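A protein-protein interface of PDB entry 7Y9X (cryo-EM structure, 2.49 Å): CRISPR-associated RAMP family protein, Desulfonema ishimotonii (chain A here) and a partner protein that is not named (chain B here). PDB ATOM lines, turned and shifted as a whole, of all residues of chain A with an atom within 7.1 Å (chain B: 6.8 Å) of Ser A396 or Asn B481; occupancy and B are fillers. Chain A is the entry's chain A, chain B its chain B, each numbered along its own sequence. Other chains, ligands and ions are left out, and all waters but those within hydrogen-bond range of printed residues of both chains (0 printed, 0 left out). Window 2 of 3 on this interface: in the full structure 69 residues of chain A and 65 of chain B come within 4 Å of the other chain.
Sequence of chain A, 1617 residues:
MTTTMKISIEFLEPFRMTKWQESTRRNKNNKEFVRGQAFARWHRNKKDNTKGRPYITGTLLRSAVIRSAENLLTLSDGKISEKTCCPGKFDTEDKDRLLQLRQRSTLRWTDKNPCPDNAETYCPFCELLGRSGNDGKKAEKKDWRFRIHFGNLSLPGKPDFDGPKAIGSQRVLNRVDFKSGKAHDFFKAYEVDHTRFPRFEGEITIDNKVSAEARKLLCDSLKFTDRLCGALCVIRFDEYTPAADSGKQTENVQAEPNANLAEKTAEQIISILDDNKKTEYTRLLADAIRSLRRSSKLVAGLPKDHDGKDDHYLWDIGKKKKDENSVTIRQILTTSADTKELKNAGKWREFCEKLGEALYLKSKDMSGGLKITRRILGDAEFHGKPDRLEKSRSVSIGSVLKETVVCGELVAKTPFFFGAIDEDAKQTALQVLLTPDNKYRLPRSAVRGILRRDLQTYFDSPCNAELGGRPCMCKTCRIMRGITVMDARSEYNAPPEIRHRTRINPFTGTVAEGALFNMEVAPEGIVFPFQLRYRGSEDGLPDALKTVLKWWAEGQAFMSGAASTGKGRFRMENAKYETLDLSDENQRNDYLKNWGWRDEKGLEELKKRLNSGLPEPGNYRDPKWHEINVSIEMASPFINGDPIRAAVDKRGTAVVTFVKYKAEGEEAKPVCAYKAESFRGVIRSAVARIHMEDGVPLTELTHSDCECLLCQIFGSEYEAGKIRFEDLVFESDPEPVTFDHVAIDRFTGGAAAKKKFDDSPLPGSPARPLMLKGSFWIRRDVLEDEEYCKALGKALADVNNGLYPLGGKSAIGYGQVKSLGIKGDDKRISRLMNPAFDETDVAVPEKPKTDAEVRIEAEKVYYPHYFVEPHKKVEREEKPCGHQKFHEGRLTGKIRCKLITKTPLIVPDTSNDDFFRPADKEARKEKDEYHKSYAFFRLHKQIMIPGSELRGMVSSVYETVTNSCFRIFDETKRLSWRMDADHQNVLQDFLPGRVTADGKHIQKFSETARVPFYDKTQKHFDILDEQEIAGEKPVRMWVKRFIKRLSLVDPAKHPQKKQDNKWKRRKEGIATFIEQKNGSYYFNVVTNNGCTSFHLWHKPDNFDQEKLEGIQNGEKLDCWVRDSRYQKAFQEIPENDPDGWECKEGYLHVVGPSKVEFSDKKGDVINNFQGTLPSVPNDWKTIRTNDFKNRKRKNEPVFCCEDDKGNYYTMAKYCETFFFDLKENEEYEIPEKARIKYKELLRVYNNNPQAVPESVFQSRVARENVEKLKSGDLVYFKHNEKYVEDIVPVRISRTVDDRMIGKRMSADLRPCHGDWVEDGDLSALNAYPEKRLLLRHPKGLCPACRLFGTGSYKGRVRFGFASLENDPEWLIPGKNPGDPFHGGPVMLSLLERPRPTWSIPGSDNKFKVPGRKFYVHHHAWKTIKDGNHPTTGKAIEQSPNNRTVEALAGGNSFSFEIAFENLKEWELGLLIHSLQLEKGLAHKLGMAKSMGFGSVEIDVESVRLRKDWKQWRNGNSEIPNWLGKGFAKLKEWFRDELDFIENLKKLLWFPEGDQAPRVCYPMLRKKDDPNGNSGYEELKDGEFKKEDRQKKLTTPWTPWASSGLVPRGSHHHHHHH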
ATOM      1  N   THR A  74     -22.422 -39.093   4.294  1.00  0.00           N
ATOM      2  CA  THR A  74     -21.521 -37.957   4.163  1.00  0.00           C
ATOM      3  C   THR A  74     -20.698 -38.051   2.883  1.00  0.00           C
ATOM      4  O   THR A  74     -20.485 -37.045   2.197  1.00  0.00           O
ATOM      5  CB  THR A  74     -20.611 -37.869   5.385  1.00  0.00           C
ATOM      6  OG1 THR A  74     -21.412 -37.826   6.569  1.00  0.00           O
ATOM      7  CG2 THR A  74     -19.771 -36.622   5.323  1.00  0.00           C
ATOM      8  N   SER A 105     -21.514 -36.581  18.424  1.00  0.00           N
ATOM      9  CA  SER A 105     -22.234 -35.668  17.551  1.00  0.00           C
ATOM     10  C   SER A 105     -22.660 -36.393  16.281  1.00  0.00           C
ATOM     11  O   SER A 105     -21.898 -37.188  15.727  1.00  0.00           O
ATOM     12  CB  SER A 105     -21.369 -34.452  17.224  1.00  0.00           C
ATOM     13  OG  SER A 105     -20.114 -34.843  16.704  1.00  0.00           O
ATOM     14  N   THR A 106     -23.890 -36.137  15.846  1.00  0.00           N
ATOM     15  CA  THR A 106     -24.394 -36.718  14.610  1.00  0.00           C
ATOM     16  C   THR A 106     -23.710 -36.079  13.407  1.00  0.00           C
ATOM     17  O   THR A 106     -23.446 -34.874  13.392  1.00  0.00           O
ATOM     18  CB  THR A 106     -25.908 -36.531  14.515  1.00  0.00           C
ATOM     19  OG1 THR A 106     -26.527 -37.041  15.700  1.00  0.00           O
ATOM     20  CG2 THR A 106     -26.470 -37.273  13.320  1.00  0.00           C
ATOM     21  N   LEU A 107     -23.412 -36.893  12.399  1.00  0.00           N
ATOM     22  CA  LEU A 107     -22.794 -36.379  11.185  1.00  0.00           C
ATOM     23  C   LEU A 107     -23.795 -35.563  10.383  1.00  0.00           C
ATOM     24  O   LEU A 107     -24.996 -35.846  10.381  1.00  0.00           O
ATOM     25  CB  LEU A 107     -22.241 -37.518  10.332  1.00  0.00           C
ATOM     26  CG  LEU A 107     -21.118 -38.346  10.955  1.00  0.00           C
ATOM     27  CD1 LEU A 107     -20.516 -39.277   9.920  1.00  0.00           C
ATOM     28  CD2 LEU A 107     -20.062 -37.454  11.573  1.00  0.00           C
ATOM     29  N   ARG A 108     -23.292 -34.545   9.692  1.00  0.00           N
ATOM     30  CA  ARG A 108     -24.124 -33.589   8.979  1.00  0.00           C
ATOM     31  C   ARG A 108     -23.782 -33.624   7.496  1.00  0.00           C
ATOM     32  O   ARG A 108     -22.613 -33.500   7.121  1.00  0.00           O
ATOM     33  CB  ARG A 108     -23.917 -32.182   9.542  1.00  0.00           C
ATOM     34  CG  ARG A 108     -25.032 -31.202   9.257  1.00  0.00           C
ATOM     35  CD  ARG A 108     -24.785 -29.922  10.026  1.00  0.00           C
ATOM     36  NE  ARG A 108     -25.942 -29.035  10.038  1.00  0.00           N
ATOM     37  CZ  ARG A 108     -26.113 -28.015   9.211  1.00  0.00           C
ATOM     38  NH1 ARG A 108     -25.231 -27.736   8.266  1.00  0.00           N
ATOM     39  NH2 ARG A 108     -27.198 -27.256   9.334  1.00  0.00           N
ATOM     40  N   TRP A 109     -24.802 -33.799   6.659  1.00  0.00           N
ATOM     41  CA  TRP A 109     -24.636 -33.727   5.214  1.00  0.00           C
ATOM     42  C   TRP A 109     -25.631 -32.795   4.540  1.00  0.00           C
ATOM     43  O   TRP A 109     -25.561 -32.634   3.318  1.00  0.00           O
ATOM     44  CB  TRP A 109     -24.751 -35.123   4.577  1.00  0.00           C
ATOM     45  CG  TRP A 109     -25.934 -35.905   5.048  1.00  0.00           C
ATOM     46  CD1 TRP A 109     -27.192 -35.876   4.530  1.00  0.00           C
ATOM     47  CD2 TRP A 109     -25.975 -36.816   6.147  1.00  0.00           C
ATOM     48  NE1 TRP A 109     -28.013 -36.720   5.229  1.00  0.00           N
ATOM     49  CE2 TRP A 109     -27.290 -37.308   6.232  1.00  0.00           C
ATOM     50  CE3 TRP A 109     -25.028 -37.262   7.072  1.00  0.00           C
ATOM     51  CZ2 TRP A 109     -27.682 -38.224   7.201  1.00  0.00           C
ATOM     52  CZ3 TRP A 109     -25.416 -38.172   8.028  1.00  0.00           C
ATOM     53  CH2 TRP A 109     -26.732 -38.647   8.085  1.00  0.00           C
ATOM     54  N   THR A 110     -26.554 -32.193   5.286  1.00  0.00           N
ATOM     55  CA  THR A 110     -27.489 -31.220   4.745  1.00  0.00           C
ATOM     56  C   THR A 110     -27.923 -30.289   5.867  1.00  0.00           C
ATOM     57  O   THR A 110     -27.765 -30.600   7.050  1.00  0.00           O
ATOM     58  CB  THR A 110     -28.709 -31.896   4.105  1.00  0.00           C
ATOM     59  OG1 THR A 110     -29.580 -30.897   3.565  1.00  0.00           O
ATOM     60  CG2 THR A 110     -29.472 -32.714   5.134  1.00  0.00           C
ATOM     61  N   ASP A 111     -28.460 -29.133   5.485  1.00  0.00           N
ATOM     62  CA  ASP A 111     -28.999 -28.176   6.442  1.00  0.00           C
ATOM     63  C   ASP A 111     -30.509 -28.277   6.594  1.00  0.00           C
ATOM     64  O   ASP A 111     -31.085 -27.547   7.405  1.00  0.00           O
ATOM     65  CB  ASP A 111     -28.630 -26.745   6.036  1.00  0.00           C
ATOM     66  CG  ASP A 111     -27.140 -26.530   5.949  1.00  0.00           C
ATOM     67  OD1 ASP A 111     -26.386 -27.505   6.145  1.00  0.00           O
ATOM     68  OD2 ASP A 111     -26.721 -25.383   5.689  1.00  0.00           O
ATOM     69  N   SER A 394     -24.859 -31.538  15.799  1.00  0.00           N
ATOM     70  CA  SER A 394     -24.729 -32.019  14.430  1.00  0.00           C
ATOM     71  C   SER A 394     -23.493 -31.379  13.822  1.00  0.00           C
ATOM     72  O   SER A 394     -23.402 -30.150  13.750  1.00  0.00           O
ATOM     73  CB  SER A 394     -25.968 -31.689  13.599  1.00  0.00           C
ATOM     74  OG  SER A 394     -27.119 -32.318  14.128  1.00  0.00           O
ATOM     75  N   VAL A 395     -22.550 -32.206  13.384  1.00  0.00           N
ATOM     76  CA  VAL A 395     -21.264 -31.738  12.882  1.00  0.00           C
ATOM     77  C   VAL A 395     -21.036 -32.322  11.496  1.00  0.00           C
ATOM     78  O   VAL A 395     -21.236 -33.521  11.282  1.00  0.00           O
ATOM     79  CB  VAL A 395     -20.112 -32.120  13.831  1.00  0.00           C
ATOM     80  CG1 VAL A 395     -18.792 -31.700  13.249  1.00  0.00           C
ATOM     81  CG2 VAL A 395     -20.316 -31.469  15.182  1.00  0.00           C
ATOM     82  N   SER A 396     -20.623 -31.476  10.559  1.00  0.00           N
ATOM     83  CA  SER A 396     -20.243 -31.913   9.225  1.00  0.00           C
ATOM     84  C   SER A 396     -18.738 -32.128   9.186  1.00  0.00           C
ATOM     85  O   SER A 396     -17.972 -31.242   9.572  1.00  0.00           O
ATOM     86  CB  SER A 396     -20.660 -30.891   8.168  1.00  0.00           C
ATOM     87  OG  SER A 396     -20.007 -29.655   8.374  1.00  0.00           O
ATOM     88  N   ILE A 397     -18.318 -33.310   8.731  1.00  0.00           N
ATOM     89  CA  ILE A 397     -16.900 -33.647   8.664  1.00  0.00           C
ATOM     90  C   ILE A 397     -16.316 -33.474   7.271  1.00  0.00           C
ATOM     91  O   ILE A 397     -15.086 -33.545   7.117  1.00  0.00           O
ATOM     92  CB  ILE A 397     -16.644 -35.088   9.157  1.00  0.00           C
ATOM     93  CG1 ILE A 397     -17.500 -36.082   8.367  1.00  0.00           C
ATOM     94  CG2 ILE A 397     -16.898 -35.194  10.651  1.00  0.00           C
ATOM     95  CD1 ILE A 397     -17.294 -37.518   8.769  1.00  0.00           C
ATOM     96  N   GLY A 398     -17.142 -33.238   6.261  1.00  0.00           N
ATOM     97  CA  GLY A 398     -16.672 -33.113   4.899  1.00  0.00           C
ATOM     98  C   GLY A 398     -16.765 -34.421   4.133  1.00  0.00           C
ATOM     99  O   GLY A 398     -16.849 -35.509   4.699  1.00  0.00           O
ATOM    100  N   SER A 399     -16.745 -34.300   2.806  1.00  0.00           N
ATOM    101  CA  SER A 399     -16.857 -35.454   1.924  1.00  0.00           C
ATOM    102  C   SER A 399     -15.524 -36.136   1.657  1.00  0.00           C
ATOM    103  O   SER A 399     -15.501 -37.143   0.945  1.00  0.00           O
ATOM    104  CB  SER A 399     -17.489 -35.043   0.592  1.00  0.00           C
ATOM    105  OG  SER A 399     -18.778 -34.493   0.781  1.00  0.00           O
ATOM    106  N   GLU B 476     -17.142 -27.565  17.680  1.00  0.00           N
ATOM    107  CA  GLU B 476     -16.783 -28.850  17.087  1.00  0.00           C
ATOM    108  C   GLU B 476     -16.640 -28.754  15.574  1.00  0.00           C
ATOM    109  O   GLU B 476     -15.702 -29.319  15.003  1.00  0.00           O
ATOM    110  CB  GLU B 476     -17.804 -29.920  17.466  1.00  0.00           C
ATOM    111  CG  GLU B 476     -17.755 -30.289  18.931  1.00  0.00           C
ATOM    112  CD  GLU B 476     -18.608 -31.489  19.260  1.00  0.00           C
ATOM    113  OE1 GLU B 476     -19.325 -31.976  18.362  1.00  0.00           O
ATOM    114  OE2 GLU B 476     -18.555 -31.947  20.419  1.00  0.00           O
ATOM    115  N   ASN B 477     -17.556 -28.051  14.906  1.00  0.00           N
ATOM    116  CA  ASN B 477     -17.397 -27.827  13.474  1.00  0.00           C
ATOM    117  C   ASN B 477     -16.143 -27.013  13.179  1.00  0.00           C
ATOM    118  O   ASN B 477     -15.518 -27.184  12.128  1.00  0.00           O
ATOM    119  CB  ASN B 477     -18.633 -27.133  12.904  1.00  0.00           C
ATOM    120  CG  ASN B 477     -19.835 -28.053  12.815  1.00  0.00           C
ATOM    121  OD1 ASN B 477     -20.015 -28.753  11.822  1.00  0.00           O
ATOM    122  ND2 ASN B 477     -20.674 -28.043  13.842  1.00  0.00           N
ATOM    123  N   TYR B 478     -15.765 -26.117  14.092  1.00  0.00           N
ATOM    124  CA  TYR B 478     -14.580 -25.290  13.886  1.00  0.00           C
ATOM    125  C   TYR B 478     -13.297 -26.095  14.054  1.00  0.00           C
ATOM    126  O   TYR B 478     -12.324 -25.882  13.322  1.00  0.00           O
ATOM    127  CB  TYR B 478     -14.619 -24.100  14.847  1.00  0.00           C
ATOM    128  CG  TYR B 478     -13.299 -23.423  15.094  1.00  0.00           C
ATOM    129  CD1 TYR B 478     -12.741 -22.576  14.150  1.00  0.00           C
ATOM    130  CD2 TYR B 478     -12.623 -23.609  16.288  1.00  0.00           C
ATOM    131  CE1 TYR B 478     -11.540 -21.954  14.380  1.00  0.00           C
ATOM    132  CE2 TYR B 478     -11.422 -22.990  16.526  1.00  0.00           C
ATOM    133  CZ  TYR B 478     -10.885 -22.164  15.570  1.00  0.00           C
ATOM    134  OH  TYR B 478      -9.684 -21.545  15.810  1.00  0.00           O
ATOM    135  N   ILE B 479     -13.271 -27.018  15.014  1.00  0.00           N
ATOM    136  CA  ILE B 479     -12.070 -27.815  15.242  1.00  0.00           C
ATOM    137  C   ILE B 479     -11.861 -28.812  14.107  1.00  0.00           C
ATOM    138  O   ILE B 479     -10.734 -29.006  13.635  1.00  0.00           O
ATOM    139  CB  ILE B 479     -12.151 -28.510  16.613  1.00  0.00           C
ATOM    140  CG1 ILE B 479     -12.058 -27.474  17.735  1.00  0.00           C
ATOM    141  CG2 ILE B 479     -11.049 -29.541  16.758  1.00  0.00           C
ATOM    142  CD1 ILE B 479     -12.213 -28.055  19.120  1.00  0.00           C
ATOM    143  N   LEU B 480     -12.933 -29.460  13.651  1.00  0.00           N
ATOM    144  CA  LEU B 480     -12.804 -30.431  12.570  1.00  0.00           C
ATOM    145  C   LEU B 480     -12.483 -29.747  11.245  1.00  0.00           C
ATOM    146  O   LEU B 480     -11.552 -30.148  10.539  1.00  0.00           O
ATOM    147  CB  LEU B 480     -14.083 -31.261  12.453  1.00  0.00           C
ATOM    148  CG  LEU B 480     -14.319 -32.225  13.617  1.00  0.00           C
ATOM    149  CD1 LEU B 480     -15.525 -33.091  13.370  1.00  0.00           C
ATOM    150  CD2 LEU B 480     -13.091 -33.079  13.866  1.00  0.00           C
ATOM    151  N   ASN B 481     -13.237 -28.708  10.894  1.00  0.00           N
ATOM    152  CA  ASN B 481     -13.080 -28.028   9.607  1.00  0.00           C
ATOM    153  C   ASN B 481     -13.207 -26.527   9.843  1.00  0.00           C
ATOM    154  O   ASN B 481     -14.292 -25.959   9.708  1.00  0.00           O
ATOM    155  CB  ASN B 481     -14.107 -28.526   8.603  1.00  0.00           C
ATOM    156  CG  ASN B 481     -15.492 -28.631   9.198  1.00  0.00           C
ATOM    157  OD1 ASN B 481     -15.841 -29.639   9.801  1.00  0.00           O
ATOM    158  ND2 ASN B 481     -16.282 -27.579   9.049  1.00  0.00           N
ATOM    159  N   GLU B 482     -12.091 -25.887  10.171  1.00  0.00           N
ATOM    160  CA  GLU B 482     -12.091 -24.449  10.370  1.00  0.00           C
ATOM    161  C   GLU B 482     -12.393 -23.736   9.060  1.00  0.00           C
ATOM    162  O   GLU B 482     -12.086 -24.236   7.974  1.00  0.00           O
ATOM    163  CB  GLU B 482     -10.747 -23.993  10.935  1.00  0.00           C
ATOM    164  CG  GLU B 482      -9.553 -24.437  10.120  1.00  0.00           C
ATOM    165  CD  GLU B 482      -8.242 -24.082  10.783  1.00  0.00           C
ATOM    166  OE1 GLU B 482      -8.276 -23.570  11.921  1.00  0.00           O
ATOM    167  OE2 GLU B 482      -7.179 -24.314  10.169  1.00  0.00           O
ATOM    168  N   GLU B 483     -13.050 -22.579   9.176  1.00  0.00           N
ATOM    169  CA  GLU B 483     -13.465 -21.726   8.064  1.00  0.00           C
ATOM    170  C   GLU B 483     -14.645 -22.333   7.312  1.00  0.00           C
ATOM    171  O   GLU B 483     -15.299 -21.647   6.521  1.00  0.00           O
ATOM    172  CB  GLU B 483     -12.305 -21.486   7.094  1.00  0.00           C
ATOM    173  CG  GLU B 483     -11.058 -20.901   7.722  1.00  0.00           C
ATOM    174  CD  GLU B 483      -9.853 -21.031   6.814  1.00  0.00           C
ATOM    175  OE1 GLU B 483      -9.977 -21.689   5.760  1.00  0.00           O
ATOM    176  OE2 GLU B 483      -8.782 -20.485   7.153  1.00  0.00           O
ATOM    177  N   GLY B 484     -14.942 -23.602   7.576  1.00  0.00           N
ATOM    178  CA  GLY B 484     -16.113 -24.248   7.021  1.00  0.00           C
ATOM    179  C   GLY B 484     -17.217 -24.201   8.047  1.00  0.00           C
ATOM    180  O   GLY B 484     -18.380 -24.506   7.766  1.00  0.00           O
ATOM    181  N   SER B 485     -16.838 -23.806   9.259  1.00  0.00           N
ATOM    182  CA  SER B 485     -17.763 -23.542  10.347  1.00  0.00           C
ATOM    183  C   SER B 485     -18.314 -22.124  10.305  1.00  0.00           C
ATOM    184  O   SER B 485     -18.872 -21.656  11.303  1.00  0.00           O
ATOM    185  CB  SER B 485     -17.070 -23.793  11.684  1.00  0.00           C
ATOM    186  OG  SER B 485     -15.900 -23.007  11.799  1.00  0.00           O
ATOM    187  N   ALA B 486     -18.165 -21.432   9.175  1.00  0.00           N
ATOM    188  CA  ALA B 486     -18.600 -20.043   9.090  1.00  0.00           C
ATOM    189  C   ALA B 486     -20.110 -19.923   9.236  1.00  0.00           C
ATOM    190  O   ALA B 486     -20.604 -18.984   9.869  1.00  0.00           O
ATOM    191  CB  ALA B 486     -18.133 -19.429   7.773  1.00  0.00           C
ATOM    192  N   PHE B 488     -22.105 -21.946  10.927  1.00  0.00           N
ATOM    193  CA  PHE B 488     -22.430 -22.162  12.332  1.00  0.00           C
ATOM    194  C   PHE B 488     -22.049 -20.965  13.191  1.00  0.00           C
ATOM    195  O   PHE B 488     -22.636 -20.759  14.257  1.00  0.00           O
ATOM    196  CB  PHE B 488     -21.745 -23.427  12.845  1.00  0.00           C
ATOM    197  CG  PHE B 488     -22.317 -24.691  12.283  1.00  0.00           C
ATOM    198  CD1 PHE B 488     -23.362 -25.333  12.922  1.00  0.00           C
ATOM    199  CD2 PHE B 488     -21.822 -25.234  11.113  1.00  0.00           C
ATOM    200  CE1 PHE B 488     -23.896 -26.494  12.408  1.00  0.00           C
ATOM    201  CE2 PHE B 488     -22.355 -26.394  10.595  1.00  0.00           C
ATOM    202  CZ  PHE B 488     -23.391 -27.023  11.244  1.00  0.00           C
ATOM    203  N   TYR B 738     -16.731 -14.507   9.034  1.00  0.00           N
ATOM    204  CA  TYR B 738     -15.834 -15.346   9.817  1.00  0.00           C
ATOM    205  C   TYR B 738     -14.470 -14.696  10.025  1.00  0.00           C
ATOM    206  O   TYR B 738     -13.793 -15.007  11.009  1.00  0.00           O
ATOM    207  CB  TYR B 738     -15.679 -16.701   9.117  1.00  0.00           C
ATOM    208  CG  TYR B 738     -14.771 -17.694   9.809  1.00  0.00           C
ATOM    209  CD1 TYR B 738     -15.260 -18.551  10.783  1.00  0.00           C
ATOM    210  CD2 TYR B 738     -13.425 -17.775   9.486  1.00  0.00           C
ATOM    211  CE1 TYR B 738     -14.435 -19.458  11.415  1.00  0.00           C
ATOM    212  CE2 TYR B 738     -12.592 -18.673  10.115  1.00  0.00           C
ATOM    213  CZ  TYR B 738     -13.101 -19.512  11.079  1.00  0.00           C
ATOM    214  OH  TYR B 738     -12.270 -20.409  11.702  1.00  0.00           O
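The side-chain amide nitrogen of Asn B481 sits at hydrogen-bond distance from the backbone carbonyl oxygen of Asn B477 (3.2 Å). The backbone carbonyl oxygen of Thr A106 lies within hydrogen-bond range of the backbone NH of Val A395 (2.8 Å). The side-chain carboxylate (OD1) of Asp A111 lies within salt-bridge range of the guanidinium group (NH1) of Arg A108 (2.4 Å). The backbone NH (N) of Arg A108 sits at hydrogen-bond distance from the backbone carbonyl oxygen (O) of Val A395, 2.8 Å away.
Among the printed residues, merely in contact across the chains: Arg A108 with Phe B488, Ser A394 with Phe B488, Val A395 with Glu B476, Val A395 with Asn B477, Val A395 with Leu B480 and Ile A397 with Leu B480.
Of the printed residues of chain B, Ser A105 touches Glu B476 (3.4 Å). Printed residues of chain B within 4 Å of Arg A108: Phe B488 (3.4 Å). Printed residues of chain B within 4 Å of Ser A394: Asn B477 and Phe B488. Of the printed residues of chain A, Glu B476 touches Ser A105 and Val A395. Printed residues of chain A within 4 Å of Leu B480: Val A395 and Ile A397. Of chain A, only Ser A396 (2.7 Å) comes within 4 Å of Asn B481. The nearest residue of chain A that does not touch Asn B481 is Ile A397 (4.3 Å).
OE1 of Glu B476 is in hydrogen-bond range of OG of Ser A105, at 3.4 Å. The side-chain amide nitrogen of Asn B477 lies within hydrogen-bond range of the backbone carbonyl oxygen of Ser A394. The backbone NH (N) of Ser A396 sits at hydrogen-bond distance from the side-chain amide oxygen (OD1) of Asn B477, 3.1 Å away. O of Ser A396 lies close to OD1 of Asn B481.
Of the 13 printed residues of chain B, 5 touch a printed residue of chain A. Hydrophobic or aromatic side chains of chain B within 4 Å of the printed part of chain A: Leu B480 and Phe B488. Printed residues of chain A that touch a printed residue of chain B: Ser A105, Arg A108, Ser A394, Val A395, Ser A396 and Ile A397. Hydrophobic or aromatic side chains of chain A that line the printed part of chain B: Val A395 and Ile A397.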
